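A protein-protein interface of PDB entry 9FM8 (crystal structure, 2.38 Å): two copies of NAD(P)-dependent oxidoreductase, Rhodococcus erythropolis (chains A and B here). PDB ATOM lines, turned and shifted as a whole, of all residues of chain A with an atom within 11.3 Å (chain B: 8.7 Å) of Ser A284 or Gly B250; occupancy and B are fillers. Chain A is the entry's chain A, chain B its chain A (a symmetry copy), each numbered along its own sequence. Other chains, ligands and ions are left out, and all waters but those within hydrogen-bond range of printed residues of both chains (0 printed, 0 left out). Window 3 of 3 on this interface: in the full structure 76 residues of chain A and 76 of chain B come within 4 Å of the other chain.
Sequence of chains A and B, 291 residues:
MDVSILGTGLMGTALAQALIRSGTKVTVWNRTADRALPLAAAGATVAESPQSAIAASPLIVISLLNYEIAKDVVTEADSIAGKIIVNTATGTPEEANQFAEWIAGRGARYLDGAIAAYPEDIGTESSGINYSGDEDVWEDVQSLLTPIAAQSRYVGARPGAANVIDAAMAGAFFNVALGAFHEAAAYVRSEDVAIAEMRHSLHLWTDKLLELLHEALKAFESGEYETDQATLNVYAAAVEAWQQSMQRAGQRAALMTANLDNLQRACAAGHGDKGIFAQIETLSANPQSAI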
ATOM      1  N   PRO A  93      34.924  -6.313 -19.860  1.00  0.00           N
ATOM      2  CA  PRO A  93      35.750  -6.386 -18.659  1.00  0.00           C
ATOM      3  C   PRO A  93      36.980  -7.260 -18.884  1.00  0.00           C
ATOM      4  O   PRO A  93      38.051  -6.934 -18.391  1.00  0.00           O
ATOM      5  CB  PRO A  93      34.791  -6.936 -17.577  1.00  0.00           C
ATOM      6  CG  PRO A  93      33.686  -7.605 -18.367  1.00  0.00           C
ATOM      7  CD  PRO A  93      33.552  -6.801 -19.651  1.00  0.00           C
ATOM      8  N   GLU A  94      36.827  -8.360 -19.631  1.00  0.00           N
ATOM      9  CA  GLU A  94      37.936  -9.253 -19.946  1.00  0.00           C
ATOM     10  C   GLU A  94      39.072  -8.462 -20.609  1.00  0.00           C
ATOM     11  O   GLU A  94      40.215  -8.507 -20.152  1.00  0.00           O
ATOM     12  CB  GLU A  94      37.482 -10.389 -20.868  1.00  0.00           C
ATOM     13  CG  GLU A  94      36.544 -11.419 -20.233  1.00  0.00           C
ATOM     14  CD  GLU A  94      35.046 -11.124 -20.156  1.00  0.00           C
ATOM     15  OE1 GLU A  94      34.460 -10.439 -21.039  1.00  0.00           O
ATOM     16  OE2 GLU A  94      34.447 -11.658 -19.194  1.00  0.00           O
ATOM     17  N   VAL A 164      31.849  -2.599 -17.390  1.00  0.00           N
ATOM     18  CA  VAL A 164      30.619  -3.311 -17.107  1.00  0.00           C
ATOM     19  C   VAL A 164      29.494  -2.287 -17.020  1.00  0.00           C
ATOM     20  O   VAL A 164      28.445  -2.439 -17.625  1.00  0.00           O
ATOM     21  CB  VAL A 164      30.753  -4.136 -15.817  1.00  0.00           C
ATOM     22  CG1 VAL A 164      29.407  -4.611 -15.288  1.00  0.00           C
ATOM     23  CG2 VAL A 164      31.689  -5.318 -16.024  1.00  0.00           C
ATOM     24  N   ASP A 261       7.144 -10.467 -21.411  1.00  0.00           N
ATOM     25  CA  ASP A 261       7.750 -11.747 -21.096  1.00  0.00           C
ATOM     26  C   ASP A 261       8.498 -11.624 -19.766  1.00  0.00           C
ATOM     27  O   ASP A 261       8.247 -12.373 -18.833  1.00  0.00           O
ATOM     28  CB  ASP A 261       8.562 -12.230 -22.287  1.00  0.00           C
ATOM     29  CG  ASP A 261       9.245 -13.580 -22.121  1.00  0.00           C
ATOM     30  OD1 ASP A 261       8.987 -14.254 -21.101  1.00  0.00           O
ATOM     31  OD2 ASP A 261      10.044 -13.942 -23.009  1.00  0.00           O
ATOM     32  N   ASN A 262       9.382 -10.637 -19.653  1.00  0.00           N
ATOM     33  CA  ASN A 262      10.121 -10.438 -18.418  1.00  0.00           C
ATOM     34  C   ASN A 262       9.178 -10.393 -17.227  1.00  0.00           C
ATOM     35  O   ASN A 262       9.526 -10.881 -16.154  1.00  0.00           O
ATOM     36  CB  ASN A 262      10.918  -9.137 -18.414  1.00  0.00           C
ATOM     37  CG  ASN A 262      12.272  -9.267 -19.065  1.00  0.00           C
ATOM     38  OD1 ASN A 262      12.719 -10.382 -19.338  1.00  0.00           O
ATOM     39  ND2 ASN A 262      12.944  -8.148 -19.291  1.00  0.00           N
ATOM     40  N   LEU A 263       8.031  -9.731 -17.419  1.00  0.00           N
ATOM     41  CA  LEU A 263       7.108  -9.438 -16.332  1.00  0.00           C
ATOM     42  C   LEU A 263       6.315 -10.685 -15.930  1.00  0.00           C
ATOM     43  O   LEU A 263       6.051 -10.896 -14.746  1.00  0.00           O
ATOM     44  CB  LEU A 263       6.190  -8.298 -16.762  1.00  0.00           C
ATOM     45  CG  LEU A 263       6.813  -6.904 -16.723  1.00  0.00           C
ATOM     46  CD1 LEU A 263       5.929  -5.852 -17.391  1.00  0.00           C
ATOM     47  CD2 LEU A 263       7.131  -6.519 -15.285  1.00  0.00           C
ATOM     48  N   ARG A 265       7.197 -13.990 -16.426  1.00  0.00           N
ATOM     49  CA  ARG A 265       8.152 -14.826 -15.727  1.00  0.00           C
ATOM     50  C   ARG A 265       8.200 -14.466 -14.245  1.00  0.00           C
ATOM     51  O   ARG A 265       8.257 -15.363 -13.405  1.00  0.00           O
ATOM     52  CB  ARG A 265       9.553 -14.681 -16.320  1.00  0.00           C
ATOM     53  CG  ARG A 265       9.678 -15.301 -17.701  1.00  0.00           C
ATOM     54  CD  ARG A 265      11.002 -14.941 -18.343  1.00  0.00           C
ATOM     55  NE  ARG A 265      11.138 -15.550 -19.669  1.00  0.00           N
ATOM     56  CZ  ARG A 265      11.772 -16.691 -19.934  1.00  0.00           C
ATOM     57  NH1 ARG A 265      12.317 -17.416 -18.967  1.00  0.00           N
ATOM     58  NH2 ARG A 265      11.841 -17.117 -21.183  1.00  0.00           N
ATOM     59  N   ALA A 266       8.192 -13.166 -13.928  1.00  0.00           N
ATOM     60  CA  ALA A 266       8.293 -12.732 -12.544  1.00  0.00           C
ATOM     61  C   ALA A 266       7.053 -13.171 -11.770  1.00  0.00           C
ATOM     62  O   ALA A 266       7.161 -13.532 -10.599  1.00  0.00           O
ATOM     63  CB  ALA A 266       8.488 -11.235 -12.458  1.00  0.00           C
ATOM     64  N   ALA A 269       6.837 -17.088 -11.416  1.00  0.00           N
ATOM     65  CA  ALA A 269       7.725 -17.496 -10.339  1.00  0.00           C
ATOM     66  C   ALA A 269       7.238 -16.933  -9.003  1.00  0.00           C
ATOM     67  O   ALA A 269       7.996 -16.902  -8.038  1.00  0.00           O
ATOM     68  CB  ALA A 269       9.141 -17.058 -10.651  1.00  0.00           C
ATOM     69  N   HIS A 271       6.009 -13.764  -7.927  1.00  0.00           N
ATOM     70  CA  HIS A 271       6.288 -12.424  -7.421  1.00  0.00           C
ATOM     71  C   HIS A 271       5.141 -11.470  -7.768  1.00  0.00           C
ATOM     72  O   HIS A 271       5.232 -10.272  -7.516  1.00  0.00           O
ATOM     73  CB  HIS A 271       7.630 -11.893  -7.948  1.00  0.00           C
ATOM     74  CG  HIS A 271       8.819 -12.668  -7.500  1.00  0.00           C
ATOM     75  ND1 HIS A 271       9.445 -12.417  -6.299  1.00  0.00           N
ATOM     76  CD2 HIS A 271       9.480 -13.677  -8.074  1.00  0.00           C
ATOM     77  CE1 HIS A 271      10.456 -13.258  -6.154  1.00  0.00           C
ATOM     78  NE2 HIS A 271      10.494 -14.034  -7.223  1.00  0.00           N
ATOM     79  N   ALA A 278      10.622  -6.257  -8.460  1.00  0.00           N
ATOM     80  CA  ALA A 278      10.902  -7.660  -8.245  1.00  0.00           C
ATOM     81  C   ALA A 278      10.995  -8.420  -9.569  1.00  0.00           C
ATOM     82  O   ALA A 278      11.249  -9.617  -9.537  1.00  0.00           O
ATOM     83  CB  ALA A 278       9.851  -8.245  -7.316  1.00  0.00           C
ATOM     84  N   GLN A 279      10.827  -7.757 -10.724  1.00  0.00           N
ATOM     85  CA  GLN A 279      11.037  -8.428 -12.012  1.00  0.00           C
ATOM     86  C   GLN A 279      12.508  -8.818 -12.230  1.00  0.00           C
ATOM     87  O   GLN A 279      12.817  -9.584 -13.151  1.00  0.00           O
ATOM     88  CB  GLN A 279      10.562  -7.641 -13.240  1.00  0.00           C
ATOM     89  CG  GLN A 279      11.381  -6.401 -13.609  1.00  0.00           C
ATOM     90  CD  GLN A 279      10.939  -5.772 -14.919  1.00  0.00           C
ATOM     91  OE1 GLN A 279      10.343  -4.685 -14.950  1.00  0.00           O
ATOM     92  NE2 GLN A 279      11.202  -6.459 -16.028  1.00  0.00           N
ATOM     93  N   ILE A 280      13.398  -8.266 -11.390  1.00  0.00           N
ATOM     94  CA  ILE A 280      14.832  -8.500 -11.436  1.00  0.00           C
ATOM     95  C   ILE A 280      15.146  -9.956 -11.088  1.00  0.00           C
ATOM     96  O   ILE A 280      16.151 -10.502 -11.543  1.00  0.00           O
ATOM     97  CB  ILE A 280      15.561  -7.515 -10.494  1.00  0.00           C
ATOM     98  CG1 ILE A 280      17.091  -7.480 -10.744  1.00  0.00           C
ATOM     99  CG2 ILE A 280      15.240  -7.799  -9.022  1.00  0.00           C
ATOM    100  CD1 ILE A 280      17.840  -6.422  -9.948  1.00  0.00           C
ATOM    101  N   GLU A 281      14.285 -10.593 -10.291  1.00  0.00           N
ATOM    102  CA  GLU A 281      14.584 -11.908  -9.745  1.00  0.00           C
ATOM    103  C   GLU A 281      14.517 -13.001 -10.809  1.00  0.00           C
ATOM    104  O   GLU A 281      14.779 -14.158 -10.500  1.00  0.00           O
ATOM    105  CB  GLU A 281      13.578 -12.249  -8.648  1.00  0.00           C
ATOM    106  CG  GLU A 281      13.661 -11.324  -7.438  1.00  0.00           C
ATOM    107  CD  GLU A 281      14.825 -11.647  -6.520  1.00  0.00           C
ATOM    108  OE1 GLU A 281      15.511 -12.650  -6.803  1.00  0.00           O
ATOM    109  OE2 GLU A 281      15.044 -10.915  -5.530  1.00  0.00           O
ATOM    110  N   THR A 282      14.158 -12.651 -12.049  1.00  0.00           N
ATOM    111  CA  THR A 282      13.830 -13.648 -13.055  1.00  0.00           C
ATOM    112  C   THR A 282      14.460 -13.280 -14.401  1.00  0.00           C
ATOM    113  O   THR A 282      13.896 -13.575 -15.459  1.00  0.00           O
ATOM    114  CB  THR A 282      12.304 -13.753 -13.135  1.00  0.00           C
ATOM    115  OG1 THR A 282      11.766 -12.490 -13.530  1.00  0.00           O
ATOM    116  CG2 THR A 282      11.707 -14.196 -11.809  1.00  0.00           C
ATOM    117  N   LEU A 283      15.647 -12.657 -14.351  1.00  0.00           N
ATOM    118  CA  LEU A 283      16.330 -12.193 -15.551  1.00  0.00           C
ATOM    119  C   LEU A 283      17.522 -13.085 -15.906  1.00  0.00           C
ATOM    120  O   LEU A 283      17.959 -13.088 -17.063  1.00  0.00           O
ATOM    121  CB  LEU A 283      16.736 -10.737 -15.344  1.00  0.00           C
ATOM    122  CG  LEU A 283      15.584  -9.725 -15.338  1.00  0.00           C
ATOM    123  CD1 LEU A 283      16.124  -8.368 -14.956  1.00  0.00           C
ATOM    124  CD2 LEU A 283      14.843  -9.654 -16.675  1.00  0.00           C
ATOM    125  N   SER A 284      18.039 -13.840 -14.918  1.00  0.00           N
ATOM    126  CA  SER A 284      18.963 -14.941 -15.171  1.00  0.00           C
ATOM    127  C   SER A 284      18.352 -15.927 -16.167  1.00  0.00           C
ATOM    128  O   SER A 284      17.162 -16.220 -16.085  1.00  0.00           O
ATOM    129  CB  SER A 284      19.337 -15.642 -13.897  1.00  0.00           C
ATOM    130  OG  SER A 284      19.710 -16.989 -14.161  1.00  0.00           O
ATOM    131  N   ALA A 285      19.179 -16.437 -17.093  1.00  0.00           N
ATOM    132  CA  ALA A 285      18.737 -17.394 -18.101  1.00  0.00           C
ATOM    133  C   ALA A 285      18.463 -18.758 -17.459  1.00  0.00           C
ATOM    134  O   ALA A 285      17.712 -19.566 -18.009  1.00  0.00           O
ATOM    135  CB  ALA A 285      19.767 -17.484 -19.212  1.00  0.00           C
ATOM    136  N   ASN A 286      19.097 -19.010 -16.302  1.00  0.00           N
ATOM    137  CA  ASN A 286      18.707 -20.079 -15.395  1.00  0.00           C
ATOM    138  C   ASN A 286      18.972 -21.440 -16.053  1.00  0.00           C
ATOM    139  O   ASN A 286      19.655 -22.264 -15.403  1.00  0.00           O
ATOM    140  CB  ASN A 286      17.258 -19.904 -14.956  1.00  0.00           C
ATOM    141  CG  ASN A 286      16.960 -20.642 -13.676  1.00  0.00           C
ATOM    142  OD1 ASN A 286      17.424 -20.237 -12.602  1.00  0.00           O
ATOM    143  ND2 ASN A 286      16.190 -21.715 -13.771  1.00  0.00           N
ATOM    144  N   HIS B 182      16.510  -2.756 -15.376  1.00  0.00           N
ATOM    145  CA  HIS B 182      16.548  -3.961 -14.570  1.00  0.00           C
ATOM    146  C   HIS B 182      17.575  -4.886 -15.212  1.00  0.00           C
ATOM    147  O   HIS B 182      18.459  -5.392 -14.531  1.00  0.00           O
ATOM    148  CB  HIS B 182      15.142  -4.577 -14.419  1.00  0.00           C
ATOM    149  CG  HIS B 182      14.215  -3.889 -13.460  1.00  0.00           C
ATOM    150  ND1 HIS B 182      13.703  -2.622 -13.659  1.00  0.00           N
ATOM    151  CD2 HIS B 182      13.718  -4.305 -12.285  1.00  0.00           C
ATOM    152  CE1 HIS B 182      12.933  -2.292 -12.633  1.00  0.00           C
ATOM    153  NE2 HIS B 182      12.936  -3.298 -11.783  1.00  0.00           N
ATOM    154  N   GLU B 183      17.465  -5.086 -16.531  1.00  0.00           N
ATOM    155  CA  GLU B 183      18.454  -5.864 -17.261  1.00  0.00           C
ATOM    156  C   GLU B 183      19.844  -5.311 -16.967  1.00  0.00           C
ATOM    157  O   GLU B 183      20.765  -6.051 -16.641  1.00  0.00           O
ATOM    158  CB  GLU B 183      18.182  -5.862 -18.760  1.00  0.00           C
ATOM    159  CG  GLU B 183      16.887  -6.586 -19.120  1.00  0.00           C
ATOM    160  CD  GLU B 183      16.756  -6.930 -20.596  1.00  0.00           C
ATOM    161  OE1 GLU B 183      17.541  -6.406 -21.433  1.00  0.00           O
ATOM    162  OE2 GLU B 183      15.859  -7.744 -20.907  1.00  0.00           O
ATOM    163  N   ALA B 186      21.055  -5.937 -13.362  1.00  0.00           N
ATOM    164  CA  ALA B 186      21.227  -7.353 -13.122  1.00  0.00           C
ATOM    165  C   ALA B 186      22.554  -7.794 -13.722  1.00  0.00           C
ATOM    166  O   ALA B 186      23.267  -8.609 -13.130  1.00  0.00           O
ATOM    167  CB  ALA B 186      20.076  -8.108 -13.724  1.00  0.00           C
ATOM    168  N   TYR B 187      22.863  -7.249 -14.906  1.00  0.00           N
ATOM    169  CA  TYR B 187      24.141  -7.514 -15.546  1.00  0.00           C
ATOM    170  C   TYR B 187      25.270  -7.057 -14.618  1.00  0.00           C
ATOM    171  O   TYR B 187      26.204  -7.815 -14.392  1.00  0.00           O
ATOM    172  CB  TYR B 187      24.242  -6.867 -16.931  1.00  0.00           C
ATOM    173  CG  TYR B 187      25.649  -6.922 -17.511  1.00  0.00           C
ATOM    174  CD1 TYR B 187      26.337  -8.125 -17.598  1.00  0.00           C
ATOM    175  CD2 TYR B 187      26.311  -5.765 -17.914  1.00  0.00           C
ATOM    176  CE1 TYR B 187      27.628  -8.183 -18.104  1.00  0.00           C
ATOM    177  CE2 TYR B 187      27.607  -5.810 -18.416  1.00  0.00           C
ATOM    178  CZ  TYR B 187      28.272  -7.024 -18.513  1.00  0.00           C
ATOM    179  OH  TYR B 187      29.545  -7.099 -19.013  1.00  0.00           O
ATOM    180  N   ARG B 189      25.378  -6.669 -11.488  1.00  0.00           N
ATOM    181  CA  ARG B 189      25.460  -7.445 -10.266  1.00  0.00           C
ATOM    182  C   ARG B 189      26.068  -8.811 -10.573  1.00  0.00           C
ATOM    183  O   ARG B 189      26.692  -9.397  -9.695  1.00  0.00           O
ATOM    184  CB  ARG B 189      24.078  -7.544  -9.613  1.00  0.00           C
ATOM    185  CG  ARG B 189      24.113  -7.902  -8.129  1.00  0.00           C
ATOM    186  CD  ARG B 189      22.720  -8.015  -7.497  1.00  0.00           C
ATOM    187  NE  ARG B 189      21.896  -8.998  -8.217  1.00  0.00           N
ATOM    188  CZ  ARG B 189      20.619  -9.298  -7.987  1.00  0.00           C
ATOM    189  NH1 ARG B 189      19.996  -8.777  -6.942  1.00  0.00           N
ATOM    190  NH2 ARG B 189      19.978 -10.132  -8.797  1.00  0.00           N
ATOM    191  N   SER B 190      25.886  -9.283 -11.816  1.00  0.00           N
ATOM    192  CA  SER B 190      26.340 -10.597 -12.245  1.00  0.00           C
ATOM    193  C   SER B 190      27.831 -10.586 -12.586  1.00  0.00           C
ATOM    194  O   SER B 190      28.430 -11.650 -12.725  1.00  0.00           O
ATOM    195  CB  SER B 190      25.510 -11.143 -13.413  1.00  0.00           C
ATOM    196  OG  SER B 190      25.733 -10.437 -14.627  1.00  0.00           O
ATOM    197  N   GLU B 191      28.425  -9.393 -12.728  1.00  0.00           N
ATOM    198  CA  GLU B 191      29.858  -9.268 -12.961  1.00  0.00           C
ATOM    199  C   GLU B 191      30.534  -8.948 -11.627  1.00  0.00           C
ATOM    200  O   GLU B 191      31.680  -8.504 -11.604  1.00  0.00           O
ATOM    201  CB  GLU B 191      30.180  -8.241 -14.054  1.00  0.00           C
ATOM    202  CG  GLU B 191      29.668  -8.590 -15.457  1.00  0.00           C
ATOM    203  CD  GLU B 191      30.544  -9.454 -16.363  1.00  0.00           C
ATOM    204  OE1 GLU B 191      31.489 -10.069 -15.829  1.00  0.00           O
ATOM    205  OE2 GLU B 191      30.319  -9.509 -17.606  1.00  0.00           O
ATOM    206  N   GLN B 243      25.066  -7.572 -25.870  1.00  0.00           N
ATOM    207  CA  GLN B 243      24.210  -8.727 -25.671  1.00  0.00           C
ATOM    208  C   GLN B 243      25.070  -9.911 -25.235  1.00  0.00           C
ATOM    209  O   GLN B 243      24.797 -10.540 -24.205  1.00  0.00           O
ATOM    210  CB  GLN B 243      23.450  -9.040 -26.960  1.00  0.00           C
ATOM    211  CG  GLN B 243      22.754 -10.400 -26.970  1.00  0.00           C
ATOM    212  CD  GLN B 243      22.508 -10.931 -28.369  1.00  0.00           C
ATOM    213  OE1 GLN B 243      23.435 -11.286 -29.114  1.00  0.00           O
ATOM    214  NE2 GLN B 243      21.236 -10.995 -28.742  1.00  0.00           N
ATOM    215  N   GLN B 244      26.100 -10.199 -26.050  1.00  0.00           N
ATOM    216  CA  GLN B 244      26.937 -11.370 -25.858  1.00  0.00           C
ATOM    217  C   GLN B 244      27.553 -11.300 -24.469  1.00  0.00           C
ATOM    218  O   GLN B 244      27.516 -12.265 -23.710  1.00  0.00           O
ATOM    219  CB  GLN B 244      27.993 -11.446 -26.959  1.00  0.00           C
ATOM    220  CG  GLN B 244      27.483 -12.102 -28.237  1.00  0.00           C
ATOM    221  CD  GLN B 244      28.204 -11.644 -29.490  1.00  0.00           C
ATOM    222  OE1 GLN B 244      29.318 -11.105 -29.440  1.00  0.00           O
ATOM    223  NE2 GLN B 244      27.567 -11.855 -30.634  1.00  0.00           N
ATOM    224  N   SER B 245      28.088 -10.121 -24.153  1.00  0.00           N
ATOM    225  CA  SER B 245      28.788  -9.925 -22.903  1.00  0.00           C
ATOM    226  C   SER B 245      27.800 -10.146 -21.763  1.00  0.00           C
ATOM    227  O   SER B 245      28.175 -10.685 -20.722  1.00  0.00           O
ATOM    228  CB  SER B 245      29.459  -8.559 -22.865  1.00  0.00           C
ATOM    229  OG  SER B 245      30.661  -8.591 -22.097  1.00  0.00           O
ATOM    230  N   MET B 246      26.541  -9.732 -21.986  1.00  0.00           N
ATOM    231  CA  MET B 246      25.483  -9.881 -20.996  1.00  0.00           C
ATOM    232  C   MET B 246      25.074 -11.341 -20.905  1.00  0.00           C
ATOM    233  O   MET B 246      24.867 -11.847 -19.801  1.00  0.00           O
ATOM    234  CB  MET B 246      24.218  -9.093 -21.353  1.00  0.00           C
ATOM    235  CG  MET B 246      24.266  -7.635 -20.960  1.00  0.00           C
ATOM    236  SD  MET B 246      22.645  -6.870 -21.135  1.00  0.00           S
ATOM    237  CE  MET B 246      22.633  -6.905 -22.925  1.00  0.00           C
ATOM    238  N   GLN B 247      24.943 -11.980 -22.076  1.00  0.00           N
ATOM    239  CA  GLN B 247      24.621 -13.393 -22.147  1.00  0.00           C
ATOM    240  C   GLN B 247      25.679 -14.238 -21.431  1.00  0.00           C
ATOM    241  O   GLN B 247      25.339 -14.972 -20.502  1.00  0.00           O
ATOM    242  CB  GLN B 247      24.315 -13.773 -23.593  1.00  0.00           C
ATOM    243  CG  GLN B 247      22.847 -14.137 -23.788  1.00  0.00           C
ATOM    244  CD  GLN B 247      22.301 -13.704 -25.125  1.00  0.00           C
ATOM    245  OE1 GLN B 247      22.951 -13.854 -26.167  1.00  0.00           O
ATOM    246  NE2 GLN B 247      21.106 -13.131 -25.095  1.00  0.00           N
ATOM    247  N   ARG B 248      26.955 -14.088 -21.821  1.00  0.00           N
ATOM    248  CA  ARG B 248      28.060 -14.790 -21.179  1.00  0.00           C
ATOM    249  C   ARG B 248      28.038 -14.602 -19.657  1.00  0.00           C
ATOM    250  O   ARG B 248      28.496 -15.470 -18.922  1.00  0.00           O
ATOM    251  CB  ARG B 248      29.408 -14.362 -21.779  1.00  0.00           C
ATOM    252  CG  ARG B 248      29.557 -14.669 -23.266  1.00  0.00           C
ATOM    253  CD  ARG B 248      31.008 -14.692 -23.738  1.00  0.00           C
ATOM    254  NE  ARG B 248      31.697 -13.468 -23.318  1.00  0.00           N
ATOM    255  CZ  ARG B 248      31.678 -12.301 -23.962  1.00  0.00           C
ATOM    256  NH1 ARG B 248      31.281 -12.224 -25.226  1.00  0.00           N
ATOM    257  NH2 ARG B 248      32.123 -11.217 -23.343  1.00  0.00           N
ATOM    258  N   ALA B 249      27.496 -13.480 -19.168  1.00  0.00           N
ATOM    259  CA  ALA B 249      27.350 -13.255 -17.737  1.00  0.00           C
ATOM    260  C   ALA B 249      26.158 -14.025 -17.154  1.00  0.00           C
ATOM    261  O   ALA B 249      25.929 -13.991 -15.939  1.00  0.00           O
ATOM    262  CB  ALA B 249      27.217 -11.768 -17.473  1.00  0.00           C
ATOM    263  N   GLY B 250      25.390 -14.707 -18.016  1.00  0.00           N
ATOM    264  CA  GLY B 250      24.244 -15.485 -17.573  1.00  0.00           C
ATOM    265  C   GLY B 250      23.032 -14.587 -17.334  1.00  0.00           C
ATOM    266  O   GLY B 250      22.550 -14.447 -16.212  1.00  0.00           O
ATOM    267  N   GLN B 251      22.571 -13.966 -18.420  1.00  0.00           N
ATOM    268  CA  GLN B 251      21.473 -13.020 -18.387  1.00  0.00           C
ATOM    269  C   GLN B 251      20.700 -13.178 -19.691  1.00  0.00           C
ATOM    270  O   GLN B 251      21.296 -13.133 -20.760  1.00  0.00           O
ATOM    271  CB  GLN B 251      21.994 -11.585 -18.290  1.00  0.00           C
ATOM    272  CG  GLN B 251      22.784 -11.256 -17.024  1.00  0.00           C
ATOM    273  CD  GLN B 251      21.918 -10.826 -15.859  1.00  0.00           C
ATOM    274  OE1 GLN B 251      20.896 -10.143 -16.019  1.00  0.00           O
ATOM    275  NE2 GLN B 251      22.338 -11.196 -14.661  1.00  0.00           N
ATOM    276  N   ARG B 252      19.385 -13.382 -19.602  1.00  0.00           N
ATOM    277  CA  ARG B 252      18.590 -13.707 -20.779  1.00  0.00           C
ATOM    278  C   ARG B 252      18.620 -12.529 -21.750  1.00  0.00           C
ATOM    279  O   ARG B 252      18.576 -12.738 -22.964  1.00  0.00           O
ATOM    280  CB  ARG B 252      17.180 -14.113 -20.335  1.00  0.00           C
ATOM    281  CG  ARG B 252      16.163 -14.425 -21.426  1.00  0.00           C
ATOM    282  CD  ARG B 252      14.808 -14.832 -20.823  1.00  0.00           C
ATOM    283  NE  ARG B 252      14.157 -13.792 -20.002  1.00  0.00           N
ATOM    284  CZ  ARG B 252      14.100 -13.725 -18.660  1.00  0.00           C
ATOM    285  NH1 ARG B 252      14.763 -14.599 -17.919  1.00  0.00           N
ATOM    286  NH2 ARG B 252      13.413 -12.766 -18.048  1.00  0.00           N
ATOM    287  N   ALA B 253      18.707 -11.305 -21.197  1.00  0.00           N
ATOM    288  CA  ALA B 253      18.998 -10.112 -21.976  1.00  0.00           C
ATOM    289  C   ALA B 253      17.997  -9.989 -23.116  1.00  0.00           C
ATOM    290  O   ALA B 253      18.370  -9.789 -24.270  1.00  0.00           O
ATOM    291  CB  ALA B 253      20.430 -10.150 -22.496  1.00  0.00           C
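No position is printed for both chains.
Of the 16 pairs that touch across the chains among the printed residues, none has its exchanged pair printed and touching as well.
Printed residues of chain B within 4 Å of Leu A283: His B182, Glu B183, Gln B251 and Arg B252.
Ser A284 touches just these residues of chain B: Gly B250 and Arg B252.
Of the printed residues of chain A, Glu B183 touches Asn A262 (3.4 Å) and Leu A283 (3.9 Å).
Printed residues of chain A within 4 Å of Gly B250: Ser A284.
Of chain A, only Leu A283 comes within 4 Å of Gln B251.
The nearest printed residue of chain A that does not touch Gly B250 is Ala A285 (4.01 Å).
The guanidinium group (NE) of Arg A265 lies within salt-bridge range of the side-chain carboxylate (OD1) of Asp A261 (2.9 Å).
The backbone NH of Asn A286 is in hydrogen-bond range of the side-chain hydroxyl of Ser A284 (3.0 Å).
NE2 of Gln B251 is in hydrogen-bond range of O of Ala B186.
OH of Tyr B187 lies within hydrogen-bond range of OE2 of Glu B191.
The side-chain hydroxyl (OG) of Ser B245 lies within hydrogen-bond range of the guanidinium group (NH2) of Arg B248 (3.3 Å).
The backbone carbonyl oxygen (O) of Met B246 lies close to the backbone NH (N) of Gln B251, at 3.4 Å.
OE2 of Glu B191 touches CG of Pro A93, at 3.9 Å.
O of Val A164 touches CE2 of Tyr B187 (3.6 Å).
Glu B191 touches Val A164.
NH2 of Arg B252 touches CD of Arg A265, at 3.3 Å.
CD2 of His B182 touches CG of Gln A279, 3.4 Å away.
Leu A283 touches His B182 (CD1 to C, 3.8 Å).
Leu A283 touches Glu B183 (CD1 to N, 3.9 Å).
Gln B251 touches Leu A283 (CA to O, 3.8 Å).
Gly B250 touches Ser A284.
Ala A285 touches Arg B252.
OE1 of Glu A94 lies within salt-bridge range of NH2 of Arg B248.
ND2 of Asn A262 lies within hydrogen-bond range of OE2 of Glu B183.
OD1 of Asn A262 lies within hydrogen-bond range of NH2 of Arg B252, at 2.8 Å.
The backbone carbonyl oxygen (O) of Thr A282 is in hydrogen-bond range of the guanidinium group (NH2) of Arg B252, at 2.8 Å.
O of Leu A283 lies within hydrogen-bond range of N of Arg B252, at 2.9 Å.
The guanidinium group (NH1) of Arg B252 is in hydrogen-bond range of the backbone carbonyl oxygen (O) of Ser A284 (3.4 Å).
Hydrophobic or aromatic side chains of chain A that line the printed part of chain B: Pro A93, Val A164 and Leu A283.
Hydrophobic or aromatic side chains of chain B within 4 Å of the printed part of chain A: His B182 and Tyr B187.
Among the printed residues, 16 pairs touch across the chains.
Among the printed residues, Asp or Glu carboxylates within 4 Å of a Lys or Arg side-chain nitrogen of the other chain: Glu A94 with Arg B248.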
